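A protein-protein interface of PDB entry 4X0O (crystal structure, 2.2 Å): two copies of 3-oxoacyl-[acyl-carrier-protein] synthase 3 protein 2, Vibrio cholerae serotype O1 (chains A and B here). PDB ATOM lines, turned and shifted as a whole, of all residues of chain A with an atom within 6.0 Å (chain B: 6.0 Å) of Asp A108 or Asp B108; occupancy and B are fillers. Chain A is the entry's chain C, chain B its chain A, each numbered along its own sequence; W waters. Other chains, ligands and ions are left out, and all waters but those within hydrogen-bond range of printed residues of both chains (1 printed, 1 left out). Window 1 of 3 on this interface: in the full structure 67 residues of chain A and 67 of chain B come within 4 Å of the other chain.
Asn A90 touches Asn B110, and with the chains exchanged Asn A110 touches Asn B90. Asn A90 touches Ala B111, and with the chains exchanged Ala A111 touches Asn B90. Phe A107 touches Leu B109, and with the chains exchanged Leu A109 touches Phe B107. Asp A108 touches Leu B109, and with the chains exchanged Leu A109 touches Asp B108. Positions printed for both chains: 77, 78, 79, 80, 81, 84, 86, 89, 90, 91, 92, 93, 106, 107, 108, 109, 110 and 111. Of the 13 pairs that touch across the chains among the printed residues, 13 have their exchanged pair printed and touching as well.
Asn A90 touches Ala B111 (ND2 to CA, 3.8 Å). Phe A107 touches Leu B109. Phe A107 touches Asn B110 (CB to O, 3.4 Å). O of Asp B108 touches O of Asp A108, 3.9 Å away. Asp A108 touches Leu B109. Leu A109 touches Phe B107. Asp B108 touches Leu A109. O of Asn A110 touches CB of Phe B107, 3.5 Å away. ND2 of Asn B90 touches CA of Ala A111 (3.8 Å).
The side-chain amide nitrogen (ND2) of Asn A90 lies within hydrogen-bond range of the backbone carbonyl oxygen (O) of Asn B110, 3.0 Å away. The backbone NH of Asn B110 lies within hydrogen-bond range of the backbone carbonyl oxygen of Asp A108, 2.9 Å away. The backbone NH (N) of Asn A110 lies within hydrogen-bond range of the backbone carbonyl oxygen (O) of Asp B108 (3.0 Å). ND2 of Asn B90 is in hydrogen-bond range of O of Asn A110 (3.0 Å).
Water W1 lies within hydrogen-bond range of ND2 of Asn B110, O of Ser A86 and OD2 of Asp A108.
Of the 18 printed residues of chain A, 6 touch a printed residue of chain B. Printed residues of chain A that touch a printed residue of chain B: Asn A90, Phe A107, Asp A108, Leu A109, Asn A110 and Ala A111.
Ala A92 touches none of the printed residues of chain B. Of the printed residues of chain B, Phe A107 touches Leu B109 (3.4 Å) and Asn B110 (3.4 Å). Asp A108 touches just these residues of chain B: Asp B108 (3.9 Å), Leu B109 (3.5 Å) and Asn B110 (2.9 Å). Of the printed residues of chain B, Leu A109 touches Phe B107 and Asp B108. Ile B77 touches none of the printed residues of chain A. Of the printed residues of chain A, Phe B107 touches Leu A109 and Asn A110. Asp B108 touches just these residues of chain A: Asp A108 (3.9 Å), Leu A109 (3.5 Å) and Asn A110 (3.0 Å). Of the printed residues of chain A, Leu B109 touches Phe A107 (3.4 Å) and Asp A108 (3.5 Å).
The backbone NH (N) of Leu A109 lies within hydrogen-bond range of the backbone carbonyl oxygen (O) of Val A79. N of Val B79 lies within hydrogen-bond range of O of Phe B107. O of Asn A90 sits at hydrogen-bond distance from OG of Ser A93, 2.6 Å away. The backbone NH (N) of Thr A81 sits at hydrogen-bond distance from the backbone carbonyl oxygen (O) of Leu A109 (3.2 Å). The backbone NH (N) of Ala A92 sits at hydrogen-bond distance from the side-chain amide oxygen (OD1) of Asn A90. N of Thr B81 lies within hydrogen-bond range of O of Leu B109 (3.2 Å).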
ATOM      1  N   ILE A  77     -35.884 -15.772 -29.254  1.00  0.00           N
ATOM      2  CA  ILE A  77     -34.867 -16.277 -28.315  1.00  0.00           C
ATOM      3  C   ILE A  77     -34.083 -15.103 -27.818  1.00  0.00           C
ATOM      4  O   ILE A  77     -33.493 -14.378 -28.603  1.00  0.00           O
ATOM      5  CB  ILE A  77     -33.901 -17.250 -29.001  1.00  0.00           C
ATOM      6  CG1 ILE A  77     -34.678 -18.372 -29.654  1.00  0.00           C
ATOM      7  CG2 ILE A  77     -32.899 -17.817 -27.989  1.00  0.00           C
ATOM      8  CD1 ILE A  77     -33.946 -19.052 -30.784  1.00  0.00           C
ATOM      9  N   ILE A  78     -34.107 -14.885 -26.506  1.00  0.00           N
ATOM     10  CA  ILE A  78     -33.303 -13.852 -25.894  1.00  0.00           C
ATOM     11  C   ILE A  78     -32.311 -14.552 -24.968  1.00  0.00           C
ATOM     12  O   ILE A  78     -32.698 -15.336 -24.107  1.00  0.00           O
ATOM     13  CB  ILE A  78     -34.165 -12.825 -25.126  1.00  0.00           C
ATOM     14  CG1 ILE A  78     -35.168 -12.151 -26.088  1.00  0.00           C
ATOM     15  CG2 ILE A  78     -33.290 -11.736 -24.529  1.00  0.00           C
ATOM     16  CD1 ILE A  78     -36.136 -11.176 -25.411  1.00  0.00           C
ATOM     17  N   VAL A  79     -31.035 -14.228 -25.130  1.00  0.00           N
ATOM     18  CA  VAL A  79     -30.044 -14.648 -24.203  1.00  0.00           C
ATOM     19  C   VAL A  79     -29.561 -13.410 -23.468  1.00  0.00           C
ATOM     20  O   VAL A  79     -28.955 -12.529 -24.061  1.00  0.00           O
ATOM     21  CB  VAL A  79     -28.881 -15.328 -24.908  1.00  0.00           C
ATOM     22  CG1 VAL A  79     -27.822 -15.753 -23.899  1.00  0.00           C
ATOM     23  CG2 VAL A  79     -29.371 -16.573 -25.656  1.00  0.00           C
ATOM     24  N   ALA A  80     -29.800 -13.369 -22.170  1.00  0.00           N
ATOM     25  CA  ALA A  80     -29.229 -12.366 -21.308  1.00  0.00           C
ATOM     26  C   ALA A  80     -27.842 -12.829 -20.819  1.00  0.00           C
ATOM     27  O   ALA A  80     -27.699 -13.874 -20.169  1.00  0.00           O
ATOM     28  CB  ALA A  80     -30.149 -12.108 -20.133  1.00  0.00           C
ATOM     29  N   THR A  81     -26.821 -12.075 -21.179  1.00  0.00           N
ATOM     30  CA  THR A  81     -25.450 -12.399 -20.782  1.00  0.00           C
ATOM     31  C   THR A  81     -24.587 -11.150 -20.893  1.00  0.00           C
ATOM     32  O   THR A  81     -24.857 -10.266 -21.712  1.00  0.00           O
ATOM     33  CB  THR A  81     -24.845 -13.502 -21.682  1.00  0.00           C
ATOM     34  OG1 THR A  81     -23.564 -13.896 -21.187  1.00  0.00           O
ATOM     35  CG2 THR A  81     -24.687 -13.025 -23.117  1.00  0.00           C
ATOM     36  N   PRO A  84     -20.594 -13.280 -23.399  1.00  0.00           N
ATOM     37  CA  PRO A  84     -20.866 -14.082 -24.589  1.00  0.00           C
ATOM     38  C   PRO A  84     -19.592 -14.619 -25.237  1.00  0.00           C
ATOM     39  O   PRO A  84     -18.571 -13.923 -25.239  1.00  0.00           O
ATOM     40  CB  PRO A  84     -21.531 -13.079 -25.526  1.00  0.00           C
ATOM     41  CG  PRO A  84     -20.936 -11.782 -25.135  1.00  0.00           C
ATOM     42  CD  PRO A  84     -20.790 -11.844 -23.659  1.00  0.00           C
ATOM     43  N   SER A  86     -18.895 -14.888 -28.241  1.00  0.00           N
ATOM     44  CA  SER A  86     -18.538 -14.008 -29.330  1.00  0.00           C
ATOM     45  C   SER A  86     -19.526 -12.866 -29.412  1.00  0.00           C
ATOM     46  O   SER A  86     -20.649 -12.972 -28.914  1.00  0.00           O
ATOM     47  CB  SER A  86     -18.566 -14.773 -30.657  1.00  0.00           C
ATOM     48  OG  SER A  86     -19.890 -15.218 -30.967  1.00  0.00           O
ATOM     49  N   PRO A  89     -21.026 -13.628 -34.436  1.00  0.00           N
ATOM     50  CA  PRO A  89     -22.420 -13.233 -34.217  1.00  0.00           C
ATOM     51  C   PRO A  89     -22.775 -13.279 -32.736  1.00  0.00           C
ATOM     52  O   PRO A  89     -21.919 -13.581 -31.906  1.00  0.00           O
ATOM     53  CB  PRO A  89     -23.232 -14.298 -34.994  1.00  0.00           C
ATOM     54  CG  PRO A  89     -22.242 -15.192 -35.651  1.00  0.00           C
ATOM     55  CD  PRO A  89     -20.936 -15.004 -34.944  1.00  0.00           C
ATOM     56  N   ASN A  90     -24.039 -13.020 -32.430  1.00  0.00           N
ATOM     57  CA  ASN A  90     -24.539 -13.139 -31.097  1.00  0.00           C
ATOM     58  C   ASN A  90     -24.657 -14.628 -30.700  1.00  0.00           C
ATOM     59  O   ASN A  90     -24.708 -15.519 -31.567  1.00  0.00           O
ATOM     60  CB  ASN A  90     -25.865 -12.370 -30.948  1.00  0.00           C
ATOM     61  CG  ASN A  90     -27.045 -13.042 -31.648  1.00  0.00           C
ATOM     62  OD1 ASN A  90     -27.109 -14.250 -31.751  1.00  0.00           O
ATOM     63  ND2 ASN A  90     -27.985 -12.250 -32.122  1.00  0.00           N
ATOM     64  N   ILE A  91     -24.694 -14.900 -29.409  1.00  0.00           N
ATOM     65  CA  ILE A  91     -24.844 -16.285 -28.980  1.00  0.00           C
ATOM     66  C   ILE A  91     -26.280 -16.789 -28.896  1.00  0.00           C
ATOM     67  O   ILE A  91     -26.476 -17.981 -28.803  1.00  0.00           O
ATOM     68  CB  ILE A  91     -24.070 -16.604 -27.701  1.00  0.00           C
ATOM     69  CG1 ILE A  91     -24.642 -15.877 -26.495  1.00  0.00           C
ATOM     70  CG2 ILE A  91     -22.583 -16.295 -27.898  1.00  0.00           C
ATOM     71  CD1 ILE A  91     -24.255 -16.562 -25.192  1.00  0.00           C
ATOM     72  N   ALA A  92     -27.283 -15.912 -28.961  1.00  0.00           N
ATOM     73  CA  ALA A  92     -28.666 -16.395 -29.120  1.00  0.00           C
ATOM     74  C   ALA A  92     -28.785 -17.191 -30.403  1.00  0.00           C
ATOM     75  O   ALA A  92     -29.487 -18.194 -30.451  1.00  0.00           O
ATOM     76  CB  ALA A  92     -29.653 -15.237 -29.120  1.00  0.00           C
ATOM     77  N   SER A  93     -28.075 -16.763 -31.444  1.00  0.00           N
ATOM     78  CA  SER A  93     -28.073 -17.506 -32.712  1.00  0.00           C
ATOM     79  C   SER A  93     -27.352 -18.860 -32.634  1.00  0.00           C
ATOM     80  O   SER A  93     -27.683 -19.815 -33.372  1.00  0.00           O
ATOM     81  CB  SER A  93     -27.484 -16.631 -33.844  1.00  0.00           C
ATOM     82  OG  SER A  93     -26.131 -16.293 -33.595  1.00  0.00           O
ATOM     83  N   ALA A 106     -33.671 -13.660 -32.724  1.00  0.00           N
ATOM     84  CA  ALA A 106     -32.653 -14.093 -31.743  1.00  0.00           C
ATOM     85  C   ALA A 106     -31.647 -12.981 -31.456  1.00  0.00           C
ATOM     86  O   ALA A 106     -30.901 -12.568 -32.349  1.00  0.00           O
ATOM     87  CB  ALA A 106     -31.938 -15.334 -32.267  1.00  0.00           C
ATOM     88  N   PHE A 107     -31.638 -12.497 -30.210  1.00  0.00           N
ATOM     89  CA  PHE A 107     -30.660 -11.501 -29.804  1.00  0.00           C
ATOM     90  C   PHE A 107     -30.143 -11.696 -28.406  1.00  0.00           C
ATOM     91  O   PHE A 107     -30.748 -12.376 -27.587  1.00  0.00           O
ATOM     92  CB  PHE A 107     -31.158 -10.065 -30.004  1.00  0.00           C
ATOM     93  CG  PHE A 107     -32.308  -9.652 -29.112  1.00  0.00           C
ATOM     94  CD1 PHE A 107     -33.610  -9.890 -29.494  1.00  0.00           C
ATOM     95  CD2 PHE A 107     -32.081  -8.957 -27.931  1.00  0.00           C
ATOM     96  CE1 PHE A 107     -34.665  -9.481 -28.706  1.00  0.00           C
ATOM     97  CE2 PHE A 107     -33.136  -8.527 -27.153  1.00  0.00           C
ATOM     98  CZ  PHE A 107     -34.422  -8.808 -27.529  1.00  0.00           C
ATOM     99  N   ASP A 108     -28.968 -11.131 -28.177  1.00  0.00           N
ATOM    100  CA  ASP A 108     -28.375 -11.075 -26.861  1.00  0.00           C
ATOM    101  C   ASP A 108     -28.739  -9.760 -26.245  1.00  0.00           C
ATOM    102  O   ASP A 108     -28.785  -8.721 -26.925  1.00  0.00           O
ATOM    103  CB  ASP A 108     -26.841 -11.182 -26.950  1.00  0.00           C
ATOM    104  CG  ASP A 108     -26.388 -12.524 -27.473  1.00  0.00           C
ATOM    105  OD1 ASP A 108     -27.255 -13.420 -27.638  1.00  0.00           O
ATOM    106  OD2 ASP A 108     -25.154 -12.686 -27.724  1.00  0.00           O
ATOM    107  N   LEU A 109     -28.996  -9.790 -24.962  1.00  0.00           N
ATOM    108  CA  LEU A 109     -29.317  -8.614 -24.225  1.00  0.00           C
ATOM    109  C   LEU A 109     -28.282  -8.486 -23.101  1.00  0.00           C
ATOM    110  O   LEU A 109     -28.053  -9.411 -22.355  1.00  0.00           O
ATOM    111  CB  LEU A 109     -30.738  -8.748 -23.672  1.00  0.00           C
ATOM    112  CG  LEU A 109     -31.345  -7.578 -22.952  1.00  0.00           C
ATOM    113  CD1 LEU A 109     -32.869  -7.697 -22.986  1.00  0.00           C
ATOM    114  CD2 LEU A 109     -30.862  -7.453 -21.519  1.00  0.00           C
ATOM    115  N   ASN A 110     -27.729  -7.301 -22.938  1.00  0.00           N
ATOM    116  CA  ASN A 110     -26.802  -7.014 -21.830  1.00  0.00           C
ATOM    117  C   ASN A 110     -27.313  -5.920 -20.904  1.00  0.00           C
ATOM    118  O   ASN A 110     -27.319  -4.744 -21.253  1.00  0.00           O
ATOM    119  CB  ASN A 110     -25.428  -6.623 -22.378  1.00  0.00           C
ATOM    120  CG  ASN A 110     -24.384  -6.444 -21.285  1.00  0.00           C
ATOM    121  OD1 ASN A 110     -24.634  -6.710 -20.099  1.00  0.00           O
ATOM    122  ND2 ASN A 110     -23.194  -6.020 -21.684  1.00  0.00           N
ATOM    123  N   ALA A 111     -27.745  -6.340 -19.718  1.00  0.00           N
ATOM    124  CA  ALA A 111     -28.014  -5.475 -18.580  1.00  0.00           C
ATOM    125  C   ALA A 111     -27.365  -6.094 -17.335  1.00  0.00           C
ATOM    126  O   ALA A 111     -27.859  -5.922 -16.226  1.00  0.00           O
ATOM    127  CB  ALA A 111     -29.511  -5.311 -18.361  1.00  0.00           C
ATOM    128  N   ILE B  77     -33.661   3.215 -22.882  1.00  0.00           N
ATOM    129  CA  ILE B  77     -32.549   3.462 -23.773  1.00  0.00           C
ATOM    130  C   ILE B  77     -32.067   2.121 -24.257  1.00  0.00           C
ATOM    131  O   ILE B  77     -31.672   1.284 -23.457  1.00  0.00           O
ATOM    132  CB  ILE B  77     -31.381   4.173 -23.058  1.00  0.00           C
ATOM    133  CG1 ILE B  77     -31.866   5.465 -22.418  1.00  0.00           C
ATOM    134  CG2 ILE B  77     -30.243   4.473 -24.026  1.00  0.00           C
ATOM    135  CD1 ILE B  77     -31.012   5.938 -21.274  1.00  0.00           C
ATOM    136  N   ILE B  78     -32.089   1.921 -25.564  1.00  0.00           N
ATOM    137  CA  ILE B  78     -31.565   0.708 -26.154  1.00  0.00           C
ATOM    138  C   ILE B  78     -30.430   1.130 -27.075  1.00  0.00           C
ATOM    139  O   ILE B  78     -30.585   2.011 -27.932  1.00  0.00           O
ATOM    140  CB  ILE B  78     -32.643  -0.084 -26.934  1.00  0.00           C
ATOM    141  CG1 ILE B  78     -33.786  -0.481 -26.006  1.00  0.00           C
ATOM    142  CG2 ILE B  78     -32.044  -1.339 -27.530  1.00  0.00           C
ATOM    143  CD1 ILE B  78     -34.949  -1.173 -26.706  1.00  0.00           C
ATOM    144  N   VAL B  79     -29.283   0.492 -26.894  1.00  0.00           N
ATOM    145  CA  VAL B  79     -28.169   0.689 -27.800  1.00  0.00           C
ATOM    146  C   VAL B  79     -27.956  -0.608 -28.530  1.00  0.00           C
ATOM    147  O   VAL B  79     -27.634  -1.624 -27.913  1.00  0.00           O
ATOM    148  CB  VAL B  79     -26.889   1.080 -27.068  1.00  0.00           C
ATOM    149  CG1 VAL B  79     -25.746   1.210 -28.043  1.00  0.00           C
ATOM    150  CG2 VAL B  79     -27.081   2.402 -26.332  1.00  0.00           C
ATOM    151  N   ALA B  80     -28.150  -0.574 -29.843  1.00  0.00           N
ATOM    152  CA  ALA B  80     -27.859  -1.697 -30.677  1.00  0.00           C
ATOM    153  C   ALA B  80     -26.400  -1.580 -31.112  1.00  0.00           C
ATOM    154  O   ALA B  80     -26.011  -0.624 -31.778  1.00  0.00           O
ATOM    155  CB  ALA B  80     -28.800  -1.746 -31.860  1.00  0.00           C
ATOM    156  N   THR B  81     -25.589  -2.563 -30.728  1.00  0.00           N
ATOM    157  CA  THR B  81     -24.188  -2.599 -31.106  1.00  0.00           C
ATOM    158  C   THR B  81     -23.662  -4.018 -30.989  1.00  0.00           C
ATOM    159  O   THR B  81     -24.165  -4.819 -30.198  1.00  0.00           O
ATOM    160  CB  THR B  81     -23.358  -1.676 -30.205  1.00  0.00           C
ATOM    161  OG1 THR B  81     -22.008  -1.624 -30.677  1.00  0.00           O
ATOM    162  CG2 THR B  81     -23.346  -2.183 -28.767  1.00  0.00           C
ATOM    163  N   PRO B  84     -19.345  -2.943 -28.412  1.00  0.00           N
ATOM    164  CA  PRO B  84     -19.426  -2.109 -27.233  1.00  0.00           C
ATOM    165  C   PRO B  84     -18.060  -1.896 -26.563  1.00  0.00           C
ATOM    166  O   PRO B  84     -17.247  -2.824 -26.536  1.00  0.00           O
ATOM    167  CB  PRO B  84     -20.328  -2.907 -26.313  1.00  0.00           C
ATOM    168  CG  PRO B  84     -20.064  -4.317 -26.687  1.00  0.00           C
ATOM    169  CD  PRO B  84     -19.873  -4.291 -28.166  1.00  0.00           C
ATOM    170  N   SER B  86     -17.375  -1.799 -23.531  1.00  0.00           N
ATOM    171  CA  SER B  86     -17.283  -2.752 -22.441  1.00  0.00           C
ATOM    172  C   SER B  86     -18.524  -3.606 -22.382  1.00  0.00           C
ATOM    173  O   SER B  86     -19.570  -3.228 -22.906  1.00  0.00           O
ATOM    174  CB  SER B  86     -17.139  -2.005 -21.119  1.00  0.00           C
ATOM    175  OG  SER B  86     -18.320  -1.241 -20.832  1.00  0.00           O
ATOM    176  N   PRO B  89     -19.886  -2.516 -17.333  1.00  0.00           N
ATOM    177  CA  PRO B  89     -21.329  -2.536 -17.609  1.00  0.00           C
ATOM    178  C   PRO B  89     -21.633  -2.390 -19.098  1.00  0.00           C
ATOM    179  O   PRO B  89     -20.711  -2.330 -19.927  1.00  0.00           O
ATOM    180  CB  PRO B  89     -21.864  -1.308 -16.847  1.00  0.00           C
ATOM    181  CG  PRO B  89     -20.691  -0.679 -16.171  1.00  0.00           C
ATOM    182  CD  PRO B  89     -19.459  -1.195 -16.851  1.00  0.00           C
ATOM    183  N   ASN B  90     -22.920  -2.327 -19.426  1.00  0.00           N
ATOM    184  CA  ASN B  90     -23.348  -2.097 -20.780  1.00  0.00           C
ATOM    185  C   ASN B  90     -23.082  -0.631 -21.178  1.00  0.00           C
ATOM    186  O   ASN B  90     -22.930   0.246 -20.312  1.00  0.00           O
ATOM    187  CB  ASN B  90     -24.818  -2.517 -20.953  1.00  0.00           C
ATOM    188  CG  ASN B  90     -25.801  -1.576 -20.278  1.00  0.00           C
ATOM    189  OD1 ASN B  90     -25.573  -0.392 -20.183  1.00  0.00           O
ATOM    190  ND2 ASN B  90     -26.915  -2.109 -19.825  1.00  0.00           N
ATOM    191  N   ILE B  91     -23.008  -0.367 -22.469  1.00  0.00           N
ATOM    192  CA  ILE B  91     -22.810   1.012 -22.904  1.00  0.00           C
ATOM    193  C   ILE B  91     -24.092   1.860 -23.018  1.00  0.00           C
ATOM    194  O   ILE B  91     -23.991   3.066 -23.105  1.00  0.00           O
ATOM    195  CB  ILE B  91     -21.959   1.128 -24.168  1.00  0.00           C
ATOM    196  CG1 ILE B  91     -22.674   0.565 -25.386  1.00  0.00           C
ATOM    197  CG2 ILE B  91     -20.604   0.458 -23.938  1.00  0.00           C
ATOM    198  CD1 ILE B  91     -22.113   1.127 -26.674  1.00  0.00           C
ATOM    199  N   ALA B  92     -25.286   1.256 -22.983  1.00  0.00           N
ATOM    200  CA  ALA B  92     -26.518   2.052 -22.837  1.00  0.00           C
ATOM    201  C   ALA B  92     -26.464   2.856 -21.537  1.00  0.00           C
ATOM    202  O   ALA B  92     -26.888   4.008 -21.505  1.00  0.00           O
ATOM    203  CB  ALA B  92     -27.746   1.175 -22.864  1.00  0.00           C
ATOM    204  N   SER B  93     -25.899   2.268 -20.483  1.00  0.00           N
ATOM    205  CA  SER B  93     -25.719   2.992 -19.199  1.00  0.00           C
ATOM    206  C   SER B  93     -24.663   4.128 -19.242  1.00  0.00           C
ATOM    207  O   SER B  93     -24.795   5.145 -18.544  1.00  0.00           O
ATOM    208  CB  SER B  93     -25.389   2.019 -18.074  1.00  0.00           C
ATOM    209  OG  SER B  93     -24.152   1.340 -18.305  1.00  0.00           O
ATOM    210  N   ALA B 106     -32.055   0.684 -19.345  1.00  0.00           N
ATOM    211  CA  ALA B 106     -30.966   0.844 -20.309  1.00  0.00           C
ATOM    212  C   ALA B 106     -30.257  -0.473 -20.577  1.00  0.00           C
ATOM    213  O   ALA B 106     -29.677  -1.089 -19.649  1.00  0.00           O
ATOM    214  CB  ALA B 106     -29.986   1.854 -19.757  1.00  0.00           C
ATOM    215  N   PHE B 107     -30.346  -0.955 -21.814  1.00  0.00           N
ATOM    216  CA  PHE B 107     -29.635  -2.166 -22.199  1.00  0.00           C
ATOM    217  C   PHE B 107     -29.028  -2.098 -23.568  1.00  0.00           C
ATOM    218  O   PHE B 107     -29.465  -1.323 -24.421  1.00  0.00           O
ATOM    219  CB  PHE B 107     -30.480  -3.441 -22.020  1.00  0.00           C
ATOM    220  CG  PHE B 107     -31.666  -3.552 -22.938  1.00  0.00           C
ATOM    221  CD1 PHE B 107     -32.887  -3.020 -22.574  1.00  0.00           C
ATOM    222  CD2 PHE B 107     -31.585  -4.289 -24.112  1.00  0.00           C
ATOM    223  CE1 PHE B 107     -33.998  -3.183 -23.371  1.00  0.00           C
ATOM    224  CE2 PHE B 107     -32.698  -4.434 -24.932  1.00  0.00           C
ATOM    225  CZ  PHE B 107     -33.901  -3.873 -24.553  1.00  0.00           C
ATOM    226  N   ASP B 108     -28.031  -2.952 -23.778  1.00  0.00           N
ATOM    227  CA  ASP B 108     -27.456  -3.170 -25.101  1.00  0.00           C
ATOM    228  C   ASP B 108     -28.133  -4.364 -25.734  1.00  0.00           C
ATOM    229  O   ASP B 108     -28.455  -5.353 -25.060  1.00  0.00           O
ATOM    230  CB  ASP B 108     -25.958  -3.441 -24.988  1.00  0.00           C
ATOM    231  CG  ASP B 108     -25.203  -2.258 -24.441  1.00  0.00           C
ATOM    232  OD1 ASP B 108     -25.831  -1.168 -24.299  1.00  0.00           O
ATOM    233  OD2 ASP B 108     -23.981  -2.401 -24.171  1.00  0.00           O
ATOM    234  N   LEU B 109     -28.332  -4.279 -27.034  1.00  0.00           N
ATOM    235  CA  LEU B 109     -28.932  -5.356 -27.783  1.00  0.00           C
ATOM    236  C   LEU B 109     -27.970  -5.729 -28.896  1.00  0.00           C
ATOM    237  O   LEU B 109     -27.478  -4.871 -29.620  1.00  0.00           O
ATOM    238  CB  LEU B 109     -30.272  -4.874 -28.347  1.00  0.00           C
ATOM    239  CG  LEU B 109     -31.141  -5.861 -29.083  1.00  0.00           C
ATOM    240  CD1 LEU B 109     -32.593  -5.367 -29.082  1.00  0.00           C
ATOM    241  CD2 LEU B 109     -30.671  -6.105 -30.510  1.00  0.00           C
ATOM    242  N   ASN B 110     -27.720  -7.005 -29.051  1.00  0.00           N
ATOM    243  CA  ASN B 110     -26.847  -7.492 -30.114  1.00  0.00           C
ATOM    244  C   ASN B 110     -27.582  -8.445 -31.057  1.00  0.00           C
ATOM    245  O   ASN B 110     -27.873  -9.583 -30.707  1.00  0.00           O
ATOM    246  CB  ASN B 110     -25.600  -8.192 -29.539  1.00  0.00           C
ATOM    247  CG  ASN B 110     -24.598  -8.608 -30.624  1.00  0.00           C
ATOM    248  OD1 ASN B 110     -24.772  -8.329 -31.807  1.00  0.00           O
ATOM    249  ND2 ASN B 110     -23.550  -9.315 -30.210  1.00  0.00           N
ATOM    250  N   ALA B 111     -27.847  -7.948 -32.248  1.00  0.00           N
ATOM    251  CA  ALA B 111     -28.302  -8.718 -33.389  1.00  0.00           C
ATOM    252  C   ALA B 111     -27.499  -8.282 -34.625  1.00  0.00           C
ATOM    253  O   ALA B 111     -28.008  -8.320 -35.740  1.00  0.00           O
ATOM    254  CB  ALA B 111     -29.803  -8.496 -33.639  1.00  0.00           C
HETATM  255  O   HOH W   1     -22.793 -10.836 -28.446  1.00  0.00           O
